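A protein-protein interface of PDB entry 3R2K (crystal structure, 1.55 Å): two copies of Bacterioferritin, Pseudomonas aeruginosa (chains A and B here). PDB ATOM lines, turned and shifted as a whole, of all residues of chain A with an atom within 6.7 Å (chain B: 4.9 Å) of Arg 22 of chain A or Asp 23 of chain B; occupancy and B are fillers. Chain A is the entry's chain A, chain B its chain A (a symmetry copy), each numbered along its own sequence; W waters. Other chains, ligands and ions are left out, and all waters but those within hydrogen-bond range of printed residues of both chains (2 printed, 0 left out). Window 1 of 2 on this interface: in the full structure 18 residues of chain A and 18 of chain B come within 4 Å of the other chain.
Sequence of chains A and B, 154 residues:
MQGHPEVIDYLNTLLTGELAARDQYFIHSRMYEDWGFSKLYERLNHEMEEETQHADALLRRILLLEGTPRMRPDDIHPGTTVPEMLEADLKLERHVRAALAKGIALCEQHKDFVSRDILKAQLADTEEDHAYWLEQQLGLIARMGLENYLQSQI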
ATOM      1  N   GLY A  17     -18.746   9.525   6.241  1.00  0.00           N
ATOM      2  CA  GLY A  17     -18.638  10.432   7.370  1.00  0.00           C
ATOM      3  C   GLY A  17     -18.376   9.694   8.669  1.00  0.00           C
ATOM      4  O   GLY A  17     -17.607  10.158   9.503  1.00  0.00           O
ATOM      5  N   GLU A  18     -19.006   8.542   8.858  1.00  0.00           N
ATOM      6  CA  GLU A  18     -18.802   7.849  10.120  1.00  0.00           C
ATOM      7  C   GLU A  18     -17.463   7.101  10.114  1.00  0.00           C
ATOM      8  O   GLU A  18     -16.832   7.000  11.152  1.00  0.00           O
ATOM      9  CB  GLU A  18     -19.990   6.943  10.451  1.00  0.00           C
ATOM     10  CG  GLU A  18     -21.240   7.749  10.675  1.00  0.00           C
ATOM     11  CD  GLU A  18     -22.483   6.911  10.803  1.00  0.00           C
ATOM     12  OE1 GLU A  18     -22.378   5.676  10.700  1.00  0.00           O
ATOM     13  OE2 GLU A  18     -23.561   7.511  10.993  1.00  0.00           O
ATOM     14  N   LEU A  19     -17.011   6.633   8.959  1.00  0.00           N
ATOM     15  CA  LEU A  19     -15.662   6.055   8.841  1.00  0.00           C
ATOM     16  C   LEU A  19     -14.614   7.116   9.215  1.00  0.00           C
ATOM     17  O   LEU A  19     -13.629   6.827   9.877  1.00  0.00           O
ATOM     18  CB  LEU A  19     -15.420   5.523   7.431  1.00  0.00           C
ATOM     19  CG  LEU A  19     -16.254   4.313   7.017  1.00  0.00           C
ATOM     20  CD1 LEU A  19     -16.063   3.996   5.532  1.00  0.00           C
ATOM     21  CD2 LEU A  19     -15.920   3.085   7.857  1.00  0.00           C
ATOM     22  N   ALA A  20     -14.833   8.353   8.766  1.00  0.00           N
ATOM     23  CA  ALA A  20     -13.968   9.455   9.152  1.00  0.00           C
ATOM     24  C   ALA A  20     -14.027   9.771  10.647  1.00  0.00           C
ATOM     25  O   ALA A  20     -12.998   9.972  11.291  1.00  0.00           O
ATOM     26  CB  ALA A  20     -14.354  10.702   8.362  1.00  0.00           C
ATOM     27  N   ALA A  21     -15.229   9.806  11.207  1.00  0.00           N
ATOM     28  CA  ALA A  21     -15.391  10.086  12.634  1.00  0.00           C
ATOM     29  C   ALA A  21     -14.619   9.032  13.444  1.00  0.00           C
ATOM     30  O   ALA A  21     -13.868   9.371  14.371  1.00  0.00           O
ATOM     31  CB  ALA A  21     -16.833  10.085  13.022  1.00  0.00           C
ATOM     32  N   ARG A  22     -14.785   7.760  13.069  1.00  0.00           N
ATOM     33  CA  ARG A  22     -14.009   6.648  13.662  1.00  0.00           C
ATOM     34  C   ARG A  22     -12.512   6.984  13.677  1.00  0.00           C
ATOM     35  O   ARG A  22     -11.834   6.884  14.716  1.00  0.00           O
ATOM     36  CB  ARG A  22     -14.306   5.345  12.906  1.00  0.00           C
ATOM     37  CG  ARG A  22     -13.320   4.218  13.129  1.00  0.00           C
ATOM     38  CD  ARG A  22     -13.401   3.163  11.999  1.00  0.00           C
ATOM     39  NE  ARG A  22     -13.010   3.760  10.726  1.00  0.00           N
ATOM     40  CZ  ARG A  22     -12.766   3.079   9.632  1.00  0.00           C
ATOM     41  NH1 ARG A  22     -12.908   1.763   9.604  1.00  0.00           N
ATOM     42  NH2 ARG A  22     -12.386   3.740   8.542  1.00  0.00           N
ATOM     43  N   ASP A  23     -11.989   7.404  12.527  1.00  0.00           N
ATOM     44  CA  ASP A  23     -10.563   7.639  12.404  1.00  0.00           C
ATOM     45  C   ASP A  23     -10.108   8.906  13.114  1.00  0.00           C
ATOM     46  O   ASP A  23      -8.996   8.943  13.625  1.00  0.00           O
ATOM     47  CB  ASP A  23     -10.146   7.610  10.938  1.00  0.00           C
ATOM     48  CG  ASP A  23     -10.213   6.202  10.351  1.00  0.00           C
ATOM     49  OD1 ASP A  23     -10.239   5.248  11.154  1.00  0.00           O
ATOM     50  OD2 ASP A  23     -10.211   6.054   9.113  1.00  0.00           O
ATOM     51  N   GLN A  24     -10.956   9.932  13.201  1.00  0.00           N
ATOM     52  CA  GLN A  24     -10.578  11.107  13.968  1.00  0.00           C
ATOM     53  C   GLN A  24     -10.503  10.784  15.478  1.00  0.00           C
ATOM     54  O   GLN A  24      -9.611  11.226  16.195  1.00  0.00           O
ATOM     55  CB  GLN A  24     -11.511  12.286  13.688  1.00  0.00           C
ATOM     56  CG  GLN A  24     -11.021  13.592  14.287  1.00  0.00           C
ATOM     57  CD  GLN A  24     -11.717  14.781  13.676  1.00  0.00           C
ATOM     58  OE1 GLN A  24     -11.645  14.988  12.470  1.00  0.00           O
ATOM     59  NE2 GLN A  24     -12.425  15.544  14.505  1.00  0.00           N
ATOM     60  N   TYR A  25     -11.440   9.987  15.957  1.00  0.00           N
ATOM     61  CA  TYR A  25     -11.389   9.554  17.350  1.00  0.00           C
ATOM     62  C   TYR A  25     -10.212   8.585  17.592  1.00  0.00           C
ATOM     63  O   TYR A  25      -9.635   8.590  18.682  1.00  0.00           O
ATOM     64  CB  TYR A  25     -12.710   8.876  17.725  1.00  0.00           C
ATOM     65  CG  TYR A  25     -13.876   9.816  17.911  1.00  0.00           C
ATOM     66  CD1 TYR A  25     -13.738  10.978  18.653  1.00  0.00           C
ATOM     67  CD2 TYR A  25     -15.122   9.496  17.430  1.00  0.00           C
ATOM     68  CE1 TYR A  25     -14.817  11.817  18.888  1.00  0.00           C
ATOM     69  CE2 TYR A  25     -16.205  10.322  17.634  1.00  0.00           C
ATOM     70  CZ  TYR A  25     -16.050  11.483  18.371  1.00  0.00           C
ATOM     71  OH  TYR A  25     -17.120  12.333  18.601  1.00  0.00           O
ATOM     72  N   PHE A  26      -9.842   7.788  16.579  1.00  0.00           N
ATOM     73  CA  PHE A  26      -8.651   6.894  16.646  1.00  0.00           C
ATOM     74  C   PHE A  26      -7.414   7.743  16.930  1.00  0.00           C
ATOM     75  O   PHE A  26      -6.689   7.532  17.920  1.00  0.00           O
ATOM     76  CB  PHE A  26      -8.508   6.145  15.297  1.00  0.00           C
ATOM     77  CG  PHE A  26      -7.635   4.900  15.300  1.00  0.00           C
ATOM     78  CD1 PHE A  26      -7.567   4.143  14.137  1.00  0.00           C
ATOM     79  CD2 PHE A  26      -6.910   4.477  16.405  1.00  0.00           C
ATOM     80  CE1 PHE A  26      -6.816   3.003  14.065  1.00  0.00           C
ATOM     81  CE2 PHE A  26      -6.186   3.321  16.350  1.00  0.00           C
ATOM     82  CZ  PHE A  26      -6.118   2.586  15.182  1.00  0.00           C
ATOM     83  N   ILE A  27      -7.147   8.734  16.084  1.00  0.00           N
ATOM     84  CA  ILE A  27      -5.957   9.544  16.297  1.00  0.00           C
ATOM     85  C   ILE A  27      -6.047  10.394  17.553  1.00  0.00           C
ATOM     86  O   ILE A  27      -5.088  10.461  18.336  1.00  0.00           O
ATOM     87  CB  ILE A  27      -5.596  10.405  15.050  1.00  0.00           C
ATOM     88  CG1 ILE A  27      -4.324  11.210  15.310  1.00  0.00           C
ATOM     89  CG2 ILE A  27      -6.711  11.332  14.654  1.00  0.00           C
ATOM     90  CD1 ILE A  27      -3.117  10.392  15.697  1.00  0.00           C
ATOM     91  N   LEU A  44     -12.494   8.584  24.230  1.00  0.00           N
ATOM     92  CA  LEU A  44     -12.453   8.652  22.771  1.00  0.00           C
ATOM     93  C   LEU A  44     -12.215   7.285  22.136  1.00  0.00           C
ATOM     94  O   LEU A  44     -12.641   7.047  21.022  1.00  0.00           O
ATOM     95  CB  LEU A  44     -11.428   9.680  22.267  1.00  0.00           C
ATOM     96  CG  LEU A  44     -11.880  11.152  22.261  1.00  0.00           C
ATOM     97  CD1 LEU A  44     -13.197  11.316  21.554  1.00  0.00           C
ATOM     98  CD2 LEU A  44     -12.008  11.729  23.642  1.00  0.00           C
ATOM     99  N   GLU A  47     -15.579   6.066  21.918  1.00  0.00           N
ATOM    100  CA  GLU A  47     -16.247   6.734  20.805  1.00  0.00           C
ATOM    101  C   GLU A  47     -15.814   6.183  19.434  1.00  0.00           C
ATOM    102  O   GLU A  47     -16.641   6.006  18.563  1.00  0.00           O
ATOM    103  CB  GLU A  47     -16.046   8.246  20.857  1.00  0.00           C
ATOM    104  CG  GLU A  47     -16.629   8.900  22.115  1.00  0.00           C
ATOM    105  CD  GLU A  47     -18.056   8.482  22.340  1.00  0.00           C
ATOM    106  OE1 GLU A  47     -18.784   8.390  21.332  1.00  0.00           O
ATOM    107  OE2 GLU A  47     -18.443   8.218  23.499  1.00  0.00           O
ATOM    108  N   MET A  48     -14.541   5.875  19.263  1.00  0.00           N
ATOM    109  CA  MET A  48     -14.075   5.180  18.055  1.00  0.00           C
ATOM    110  C   MET A  48     -14.837   3.876  17.838  1.00  0.00           C
ATOM    111  O   MET A  48     -15.261   3.579  16.716  1.00  0.00           O
ATOM    112  CB  MET A  48     -12.584   4.849  18.148  1.00  0.00           C
ATOM    113  CG  MET A  48     -12.089   4.143  16.927  1.00  0.00           C
ATOM    114  SD  MET A  48     -10.344   3.782  16.973  1.00  0.00           S
ATOM    115  CE  MET A  48     -10.315   2.475  18.191  1.00  0.00           C
ATOM    116  N   GLU A  49     -14.999   3.075  18.888  1.00  0.00           N
ATOM    117  CA  GLU A  49     -15.744   1.822  18.785  1.00  0.00           C
ATOM    118  C   GLU A  49     -17.208   2.077  18.422  1.00  0.00           C
ATOM    119  O   GLU A  49     -17.776   1.368  17.587  1.00  0.00           O
ATOM    120  CB  GLU A  49     -15.630   1.026  20.113  1.00  0.00           C
ATOM    121  CG  GLU A  49     -14.201   0.649  20.399  1.00  0.00           C
ATOM    122  CD  GLU A  49     -13.952   0.049  21.795  1.00  0.00           C
ATOM    123  OE1 GLU A  49     -14.800   0.210  22.703  1.00  0.00           O
ATOM    124  OE2 GLU A  49     -12.873  -0.567  21.977  1.00  0.00           O
ATOM    125  N   GLU A  51     -18.423   4.671  16.752  1.00  0.00           N
ATOM    126  CA  GLU A  51     -18.536   5.097  15.352  1.00  0.00           C
ATOM    127  C   GLU A  51     -18.321   3.916  14.404  1.00  0.00           C
ATOM    128  O   GLU A  51     -18.896   3.864  13.326  1.00  0.00           O
ATOM    129  CB  GLU A  51     -17.534   6.204  15.011  1.00  0.00           C
ATOM    130  CG  GLU A  51     -17.698   7.471  15.756  1.00  0.00           C
ATOM    131  CD  GLU A  51     -18.972   8.190  15.430  1.00  0.00           C
ATOM    132  OE1 GLU A  51     -19.635   7.838  14.439  1.00  0.00           O
ATOM    133  OE2 GLU A  51     -19.256   9.160  16.143  1.00  0.00           O
ATOM    134  N   THR A  52     -17.461   2.967  14.774  1.00  0.00           N
ATOM    135  CA  THR A  52     -17.287   1.750  13.970  1.00  0.00           C
ATOM    136  C   THR A  52     -18.600   0.982  13.909  1.00  0.00           C
ATOM    137  O   THR A  52     -18.993   0.485  12.865  1.00  0.00           O
ATOM    138  CB  THR A  52     -16.157   0.871  14.536  1.00  0.00           C
ATOM    139  OG1 THR A  52     -14.958   1.643  14.629  1.00  0.00           O
ATOM    140  CG2 THR A  52     -15.906  -0.317  13.655  1.00  0.00           C
ATOM    141  N   ALA A  55     -20.932   2.941  11.607  1.00  0.00           N
ATOM    142  CA  ALA A  55     -20.546   2.672  10.223  1.00  0.00           C
ATOM    143  C   ALA A  55     -21.008   1.274   9.792  1.00  0.00           C
ATOM    144  O   ALA A  55     -21.537   1.079   8.703  1.00  0.00           O
ATOM    145  CB  ALA A  55     -19.026   2.800  10.060  1.00  0.00           C
ATOM    146  N   LEU A  59     -23.284   0.288   6.588  1.00  0.00           N
ATOM    147  CA  LEU A  59     -22.726  -0.597   5.584  1.00  0.00           C
ATOM    148  C   LEU A  59     -23.638  -1.791   5.361  1.00  0.00           C
ATOM    149  O   LEU A  59     -23.968  -2.134   4.219  1.00  0.00           O
ATOM    150  CB  LEU A  59     -21.334  -1.018   6.065  1.00  0.00           C
ATOM    151  CG  LEU A  59     -20.389  -1.755   5.134  1.00  0.00           C
ATOM    152  CD1 LEU A  59     -18.966  -1.798   5.769  1.00  0.00           C
ATOM    153  CD2 LEU A  59     -20.934  -3.127   4.842  1.00  0.00           C
ATOM    154  N   MET A  71     -16.332   3.003   0.786  1.00  0.00           N
ATOM    155  CA  MET A  71     -15.457   2.779   1.953  1.00  0.00           C
ATOM    156  C   MET A  71     -14.341   3.805   2.154  1.00  0.00           C
ATOM    157  O   MET A  71     -13.591   3.757   3.118  1.00  0.00           O
ATOM    158  CB  MET A  71     -14.843   1.388   1.876  1.00  0.00           C
ATOM    159  CG  MET A  71     -15.852   0.258   1.891  1.00  0.00           C
ATOM    160  SD  MET A  71     -16.873   0.202   3.377  1.00  0.00           S
ATOM    161  CE  MET A  71     -15.641  -0.108   4.650  1.00  0.00           C
ATOM    162  N   ARG A  72     -14.243   4.792   1.268  1.00  0.00           N
ATOM    163  CA  ARG A  72     -13.272   5.867   1.458  1.00  0.00           C
ATOM    164  C   ARG A  72     -13.748   6.863   2.513  1.00  0.00           C
ATOM    165  O   ARG A  72     -14.747   7.557   2.315  1.00  0.00           O
ATOM    166  CB  ARG A  72     -13.055   6.619   0.139  1.00  0.00           C
ATOM    167  CG  ARG A  72     -11.936   7.602   0.213  1.00  0.00           C
ATOM    168  CD  ARG A  72     -11.801   8.432  -1.085  1.00  0.00           C
ATOM    169  NE  ARG A  72     -12.792   9.485  -1.126  1.00  0.00           N
ATOM    170  CZ  ARG A  72     -12.808  10.449  -2.043  1.00  0.00           C
ATOM    171  NH1 ARG A  72     -11.876  10.487  -2.988  1.00  0.00           N
ATOM    172  NH2 ARG A  72     -13.757  11.366  -2.011  1.00  0.00           N
ATOM    173  N   PRO A  73     -13.044   6.949   3.656  1.00  0.00           N
ATOM    174  CA  PRO A  73     -13.467   7.920   4.657  1.00  0.00           C
ATOM    175  C   PRO A  73     -13.352   9.348   4.174  1.00  0.00           C
ATOM    176  O   PRO A  73     -12.455   9.660   3.385  1.00  0.00           O
ATOM    177  CB  PRO A  73     -12.505   7.691   5.832  1.00  0.00           C
ATOM    178  CG  PRO A  73     -11.904   6.333   5.582  1.00  0.00           C
ATOM    179  CD  PRO A  73     -11.858   6.189   4.085  1.00  0.00           C
ATOM    180  N   ILE A  76     -10.283  13.855   7.633  1.00  0.00           N
ATOM    181  CA  ILE A  76     -10.382  14.227   9.026  1.00  0.00           C
ATOM    182  C   ILE A  76      -9.521  15.448   9.283  1.00  0.00           C
ATOM    183  O   ILE A  76      -8.694  15.837   8.442  1.00  0.00           O
ATOM    184  CB  ILE A  76      -9.997  13.071   9.985  1.00  0.00           C
ATOM    185  CG1 ILE A  76      -8.544  12.646   9.793  1.00  0.00           C
ATOM    186  CG2 ILE A  76     -10.974  11.886   9.816  1.00  0.00           C
ATOM    187  CD1 ILE A  76      -8.005  11.828  11.002  1.00  0.00           C
ATOM    188  N   LEU A  92     -17.149  18.133  14.042  1.00  0.00           N
ATOM    189  CA  LEU A  92     -17.501  16.916  13.323  1.00  0.00           C
ATOM    190  C   LEU A  92     -18.856  16.363  13.768  1.00  0.00           C
ATOM    191  O   LEU A  92     -19.696  16.054  12.922  1.00  0.00           O
ATOM    192  CB  LEU A  92     -16.400  15.853  13.456  1.00  0.00           C
ATOM    193  CG  LEU A  92     -16.614  14.606  12.573  1.00  0.00           C
ATOM    194  CD1 LEU A  92     -17.094  14.935  11.156  1.00  0.00           C
ATOM    195  CD2 LEU A  92     -15.323  13.848  12.457  1.00  0.00           C
ATOM    196  N   LEU B  19      -4.535   0.694   7.680  1.00  0.00           N
ATOM    197  CA  LEU B  19      -5.875   1.297   7.764  1.00  0.00           C
ATOM    198  C   LEU B  19      -6.722   0.834   6.568  1.00  0.00           C
ATOM    199  O   LEU B  19      -7.901   0.545   6.701  1.00  0.00           O
ATOM    200  CB  LEU B  19      -5.785   2.819   7.813  1.00  0.00           C
ATOM    201  CG  LEU B  19      -5.157   3.415   9.071  1.00  0.00           C
ATOM    202  CD1 LEU B  19      -4.948   4.924   8.918  1.00  0.00           C
ATOM    203  CD2 LEU B  19      -5.998   3.130  10.310  1.00  0.00           C
ATOM    204  N   ALA B  20      -6.106   0.785   5.385  1.00  0.00           N
ATOM    205  CA  ALA B  20      -6.778   0.257   4.211  1.00  0.00           C
ATOM    206  C   ALA B  20      -7.112  -1.231   4.325  1.00  0.00           C
ATOM    207  O   ALA B  20      -8.217  -1.657   3.992  1.00  0.00           O
ATOM    208  CB  ALA B  20      -5.900   0.479   2.982  1.00  0.00           C
ATOM    209  N   ALA B  21      -6.164  -2.024   4.807  1.00  0.00           N
ATOM    210  CA  ALA B  21      -6.389  -3.460   4.969  1.00  0.00           C
ATOM    211  C   ALA B  21      -7.588  -3.679   5.907  1.00  0.00           C
ATOM    212  O   ALA B  21      -8.491  -4.474   5.605  1.00  0.00           O
ATOM    213  CB  ALA B  21      -5.175  -4.138   5.513  1.00  0.00           C
ATOM    214  N   ARG B  22      -7.604  -2.949   7.026  1.00  0.00           N
ATOM    215  CA  ARG B  22      -8.752  -2.948   7.960  1.00  0.00           C
ATOM    216  C   ARG B  22     -10.066  -2.739   7.196  1.00  0.00           C
ATOM    217  O   ARG B  22     -11.034  -3.506   7.348  1.00  0.00           O
ATOM    218  CB  ARG B  22      -8.536  -1.888   9.049  1.00  0.00           C
ATOM    219  CG  ARG B  22      -9.768  -1.496   9.836  1.00  0.00           C
ATOM    220  CD  ARG B  22      -9.583  -0.127  10.536  1.00  0.00           C
ATOM    221  NE  ARG B  22      -9.420   0.927   9.539  1.00  0.00           N
ATOM    222  CZ  ARG B  22      -9.463   2.211   9.806  1.00  0.00           C
ATOM    223  NH1 ARG B  22      -9.616   2.643  11.047  1.00  0.00           N
ATOM    224  NH2 ARG B  22      -9.332   3.074   8.802  1.00  0.00           N
ATOM    225  N   ASP B  23     -10.103  -1.709   6.354  1.00  0.00           N
ATOM    226  CA  ASP B  23     -11.333  -1.355   5.669  1.00  0.00           C
ATOM    227  C   ASP B  23     -11.688  -2.327   4.553  1.00  0.00           C
ATOM    228  O   ASP B  23     -12.865  -2.558   4.309  1.00  0.00           O
ATOM    229  CB  ASP B  23     -11.274   0.090   5.189  1.00  0.00           C
ATOM    230  CG  ASP B  23     -11.347   1.082   6.347  1.00  0.00           C
ATOM    231  OD1 ASP B  23     -11.783   0.658   7.437  1.00  0.00           O
ATOM    232  OD2 ASP B  23     -11.002   2.265   6.163  1.00  0.00           O
ATOM    233  N   GLN B  24     -10.701  -2.938   3.896  1.00  0.00           N
ATOM    234  CA  GLN B  24     -11.024  -3.948   2.901  1.00  0.00           C
ATOM    235  C   GLN B  24     -11.629  -5.206   3.564  1.00  0.00           C
ATOM    236  O   GLN B  24     -12.576  -5.810   3.070  1.00  0.00           O
ATOM    237  CB  GLN B  24      -9.812  -4.292   2.035  1.00  0.00           C
ATOM    238  CG  GLN B  24     -10.157  -5.167   0.843  1.00  0.00           C
ATOM    239  CD  GLN B  24      -9.059  -5.159  -0.190  1.00  0.00           C
ATOM    240  OE1 GLN B  24      -8.710  -4.107  -0.713  1.00  0.00           O
ATOM    241  NE2 GLN B  24      -8.488  -6.331  -0.458  1.00  0.00           N
ATOM    242  N   TYR B  25     -11.087  -5.589   4.705  1.00  0.00           N
ATOM    243  CA  TYR B  25     -11.659  -6.709   5.446  1.00  0.00           C
ATOM    244  C   TYR B  25     -13.038  -6.345   6.035  1.00  0.00           C
ATOM    245  O   TYR B  25     -13.905  -7.216   6.135  1.00  0.00           O
ATOM    246  CB  TYR B  25     -10.703  -7.122   6.570  1.00  0.00           C
ATOM    247  CG  TYR B  25      -9.472  -7.866   6.115  1.00  0.00           C
ATOM    248  CD1 TYR B  25      -9.567  -8.902   5.200  1.00  0.00           C
ATOM    249  CD2 TYR B  25      -8.243  -7.597   6.666  1.00  0.00           C
ATOM    250  CE1 TYR B  25      -8.453  -9.638   4.823  1.00  0.00           C
ATOM    251  CE2 TYR B  25      -7.119  -8.301   6.294  1.00  0.00           C
ATOM    252  CZ  TYR B  25      -7.229  -9.328   5.374  1.00  0.00           C
ATOM    253  OH  TYR B  25      -6.119 -10.062   4.983  1.00  0.00           O
ATOM    254  N   PHE B  26     -13.247  -5.069   6.390  1.00  0.00           N
ATOM    255  CA  PHE B  26     -14.569  -4.566   6.861  1.00  0.00           C
ATOM    256  C   PHE B  26     -15.612  -4.833   5.776  1.00  0.00           C
ATOM    257  O   PHE B  26     -16.633  -5.507   6.003  1.00  0.00           O
ATOM    258  CB  PHE B  26     -14.455  -3.049   7.155  1.00  0.00           C
ATOM    259  CG  PHE B  26     -15.543  -2.442   8.028  1.00  0.00           C
ATOM    260  CD1 PHE B  26     -15.417  -1.109   8.399  1.00  0.00           C
ATOM    261  CD2 PHE B  26     -16.647  -3.151   8.478  1.00  0.00           C
ATOM    262  CE1 PHE B  26     -16.345  -0.495   9.194  1.00  0.00           C
ATOM    263  CE2 PHE B  26     -17.558  -2.553   9.300  1.00  0.00           C
ATOM    264  CZ  PHE B  26     -17.426  -1.223   9.651  1.00  0.00           C
ATOM    265  N   ILE B  27     -15.378  -4.328   4.568  1.00  0.00           N
ATOM    266  CA  ILE B  27     -16.363  -4.528   3.516  1.00  0.00           C
ATOM    267  C   ILE B  27     -16.475  -5.981   3.090  1.00  0.00           C
ATOM    268  O   ILE B  27     -17.588  -6.507   2.937  1.00  0.00           O
ATOM    269  CB  ILE B  27     -16.121  -3.592   2.294  1.00  0.00           C
ATOM    270  CG1 ILE B  27     -17.198  -3.814   1.234  1.00  0.00           C
ATOM    271  CG2 ILE B  27     -14.761  -3.787   1.685  1.00  0.00           C
ATOM    272  CD1 ILE B  27     -18.617  -3.626   1.712  1.00  0.00           C
ATOM    273  N   PRO B  73      -6.506   6.333   4.802  1.00  0.00           N
ATOM    274  CA  PRO B  73      -6.205   4.998   4.301  1.00  0.00           C
ATOM    275  C   PRO B  73      -5.845   4.990   2.833  1.00  0.00           C
ATOM    276  O   PRO B  73      -6.362   5.810   2.068  1.00  0.00           O
ATOM    277  CB  PRO B  73      -7.507   4.213   4.520  1.00  0.00           C
ATOM    278  CG  PRO B  73      -8.290   5.029   5.514  1.00  0.00           C
ATOM    279  CD  PRO B  73      -7.905   6.458   5.245  1.00  0.00           C
ATOM    280  N   ILE B  76      -8.738   1.005  -1.344  1.00  0.00           N
ATOM    281  CA  ILE B  76      -8.991  -0.417  -1.294  1.00  0.00           C
ATOM    282  C   ILE B  76      -9.594  -0.867  -2.610  1.00  0.00           C
ATOM    283  O   ILE B  76     -10.013  -0.041  -3.438  1.00  0.00           O
ATOM    284  CB  ILE B  76      -9.900  -0.824  -0.106  1.00  0.00           C
ATOM    285  CG1 ILE B  76     -11.281  -0.182  -0.212  1.00  0.00           C
ATOM    286  CG2 ILE B  76      -9.209  -0.492   1.236  1.00  0.00           C
ATOM    287  CD1 ILE B  76     -12.333  -0.896   0.684  1.00  0.00           C
HETATM  288  O   HOH W   1     -10.268   1.903  13.801  1.00  0.00           O
HETATM  289  O   HOH W   2     -11.058   2.885   3.535  1.00  0.00           O
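OD1 of Asp 23 of chain B lies within salt-bridge range of NE of Arg 22 of chain B.
O of Leu 19 of chain A is in hydrogen-bond range of NE of Arg 22 of chain A, at 3.2 Å.
O of Met 48 of chain A is in hydrogen-bond range of OG1 of Thr 52 of chain A.
The guanidinium group (NE) of Arg 22 of chain B lies within hydrogen-bond range of the backbone carbonyl oxygen (O) of Leu 19 of chain B, at 3.2 Å.
NE of Arg 22 of chain A is in salt-bridge range of OD1 of Asp 23 of chain A (3.2 Å).
Leu 19 of chain A touches Phe 26 of chain B, and with the chains exchanged Phe 26 of chain A touches Leu 19 of chain B.
Arg 22 of chain A touches Asp 23 of chain B, and with the chains exchanged Asp 23 of chain A touches Arg 22 of chain B.
Arg 22 of chain A touches Phe 26 of chain B, and with the chains exchanged Phe 26 of chain A touches Arg 22 of chain B.
Pro 73 of chain A touches its own counterpart, Pro 73 of chain B.
11 positions are printed for both chains.
Of the 15 pairs that touch across the chains among the printed residues, 8 have their exchanged pair printed and touching as well.
OD1 of Asp 23 of chain A is in salt-bridge range of NH1 of Arg 22 of chain B (2.7 Å).
The guanidinium group (NH1) of Arg 22 of chain A lies within salt-bridge range of the side-chain carboxylate (OD1) of Asp 23 of chain B (2.7 Å).
NH2 of Arg 22 of chain A lies close to NH2 of Arg 22 of chain B.
Along chain B the printed residues that touch a printed residue of chain A span positions 19 to 76.
Of the 24 printed residues of chain A, 8 touch a printed residue of chain B.
Hydrophobic or aromatic side chains of chain A that line the printed part of chain B: Leu 19, Phe 26, Leu 59, Met 71 and Pro 73.
Printed residues of chain B within 4 Å of Arg 22 of chain A: Arg 22 (3.1 Å), Asp 23 (2.7 Å) and Phe 26 (3.999 Å).
Asp 23 of chain B touches just these residues of chain A: Arg 22 (2.7 Å) and Met 71 (3.7 Å).
Of the printed residues of chain B, Thr 52 of chain A touches Phe 26 (3.96 Å).
Of the printed residues of chain B, Asp 23 of chain A touches Arg 22.
Of the printed residues of chain B, Pro 73 of chain A touches Pro 73.
The nearest printed residue of chain B that does not touch Arg 22 of chain A is Pro 73 of chain B (5.3 Å).
Phe 26 of chain B touches Leu 19 of chain A.
Arg 22 of chain A touches Phe 26 of chain B.
Leu 19 of chain B touches Phe 26 of chain A.
Leu 59 of chain A touches Phe 26 of chain B.
Leu 59 of chain A touches Ile 27 of chain B (CD2 to CD1, 3.9 Å).
O of Asp 23 of chain B touches CE of Met 71 of chain A, 3.7 Å away.
Phe 26 of chain B touches Met 71 of chain A.
CG of Met 71 of chain A touches CB of Ile 27 of chain B, at 3.9 Å.
Met 71 of chain A touches Ile 76 of chain B.
CG of Pro 73 of chain B touches CG of Pro 73 of chain A, at 3.8 Å.
Water W2 lies within hydrogen-bond range of OD2 of Asp 23 of chain B (2.7 Å) and O of Met 71 of chain A (2.7 Å).
Water W1 lies within hydrogen-bond range of the guanidinium group of Arg 22 of chain B and the side-chain sulfur of Met 48 of chain A.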
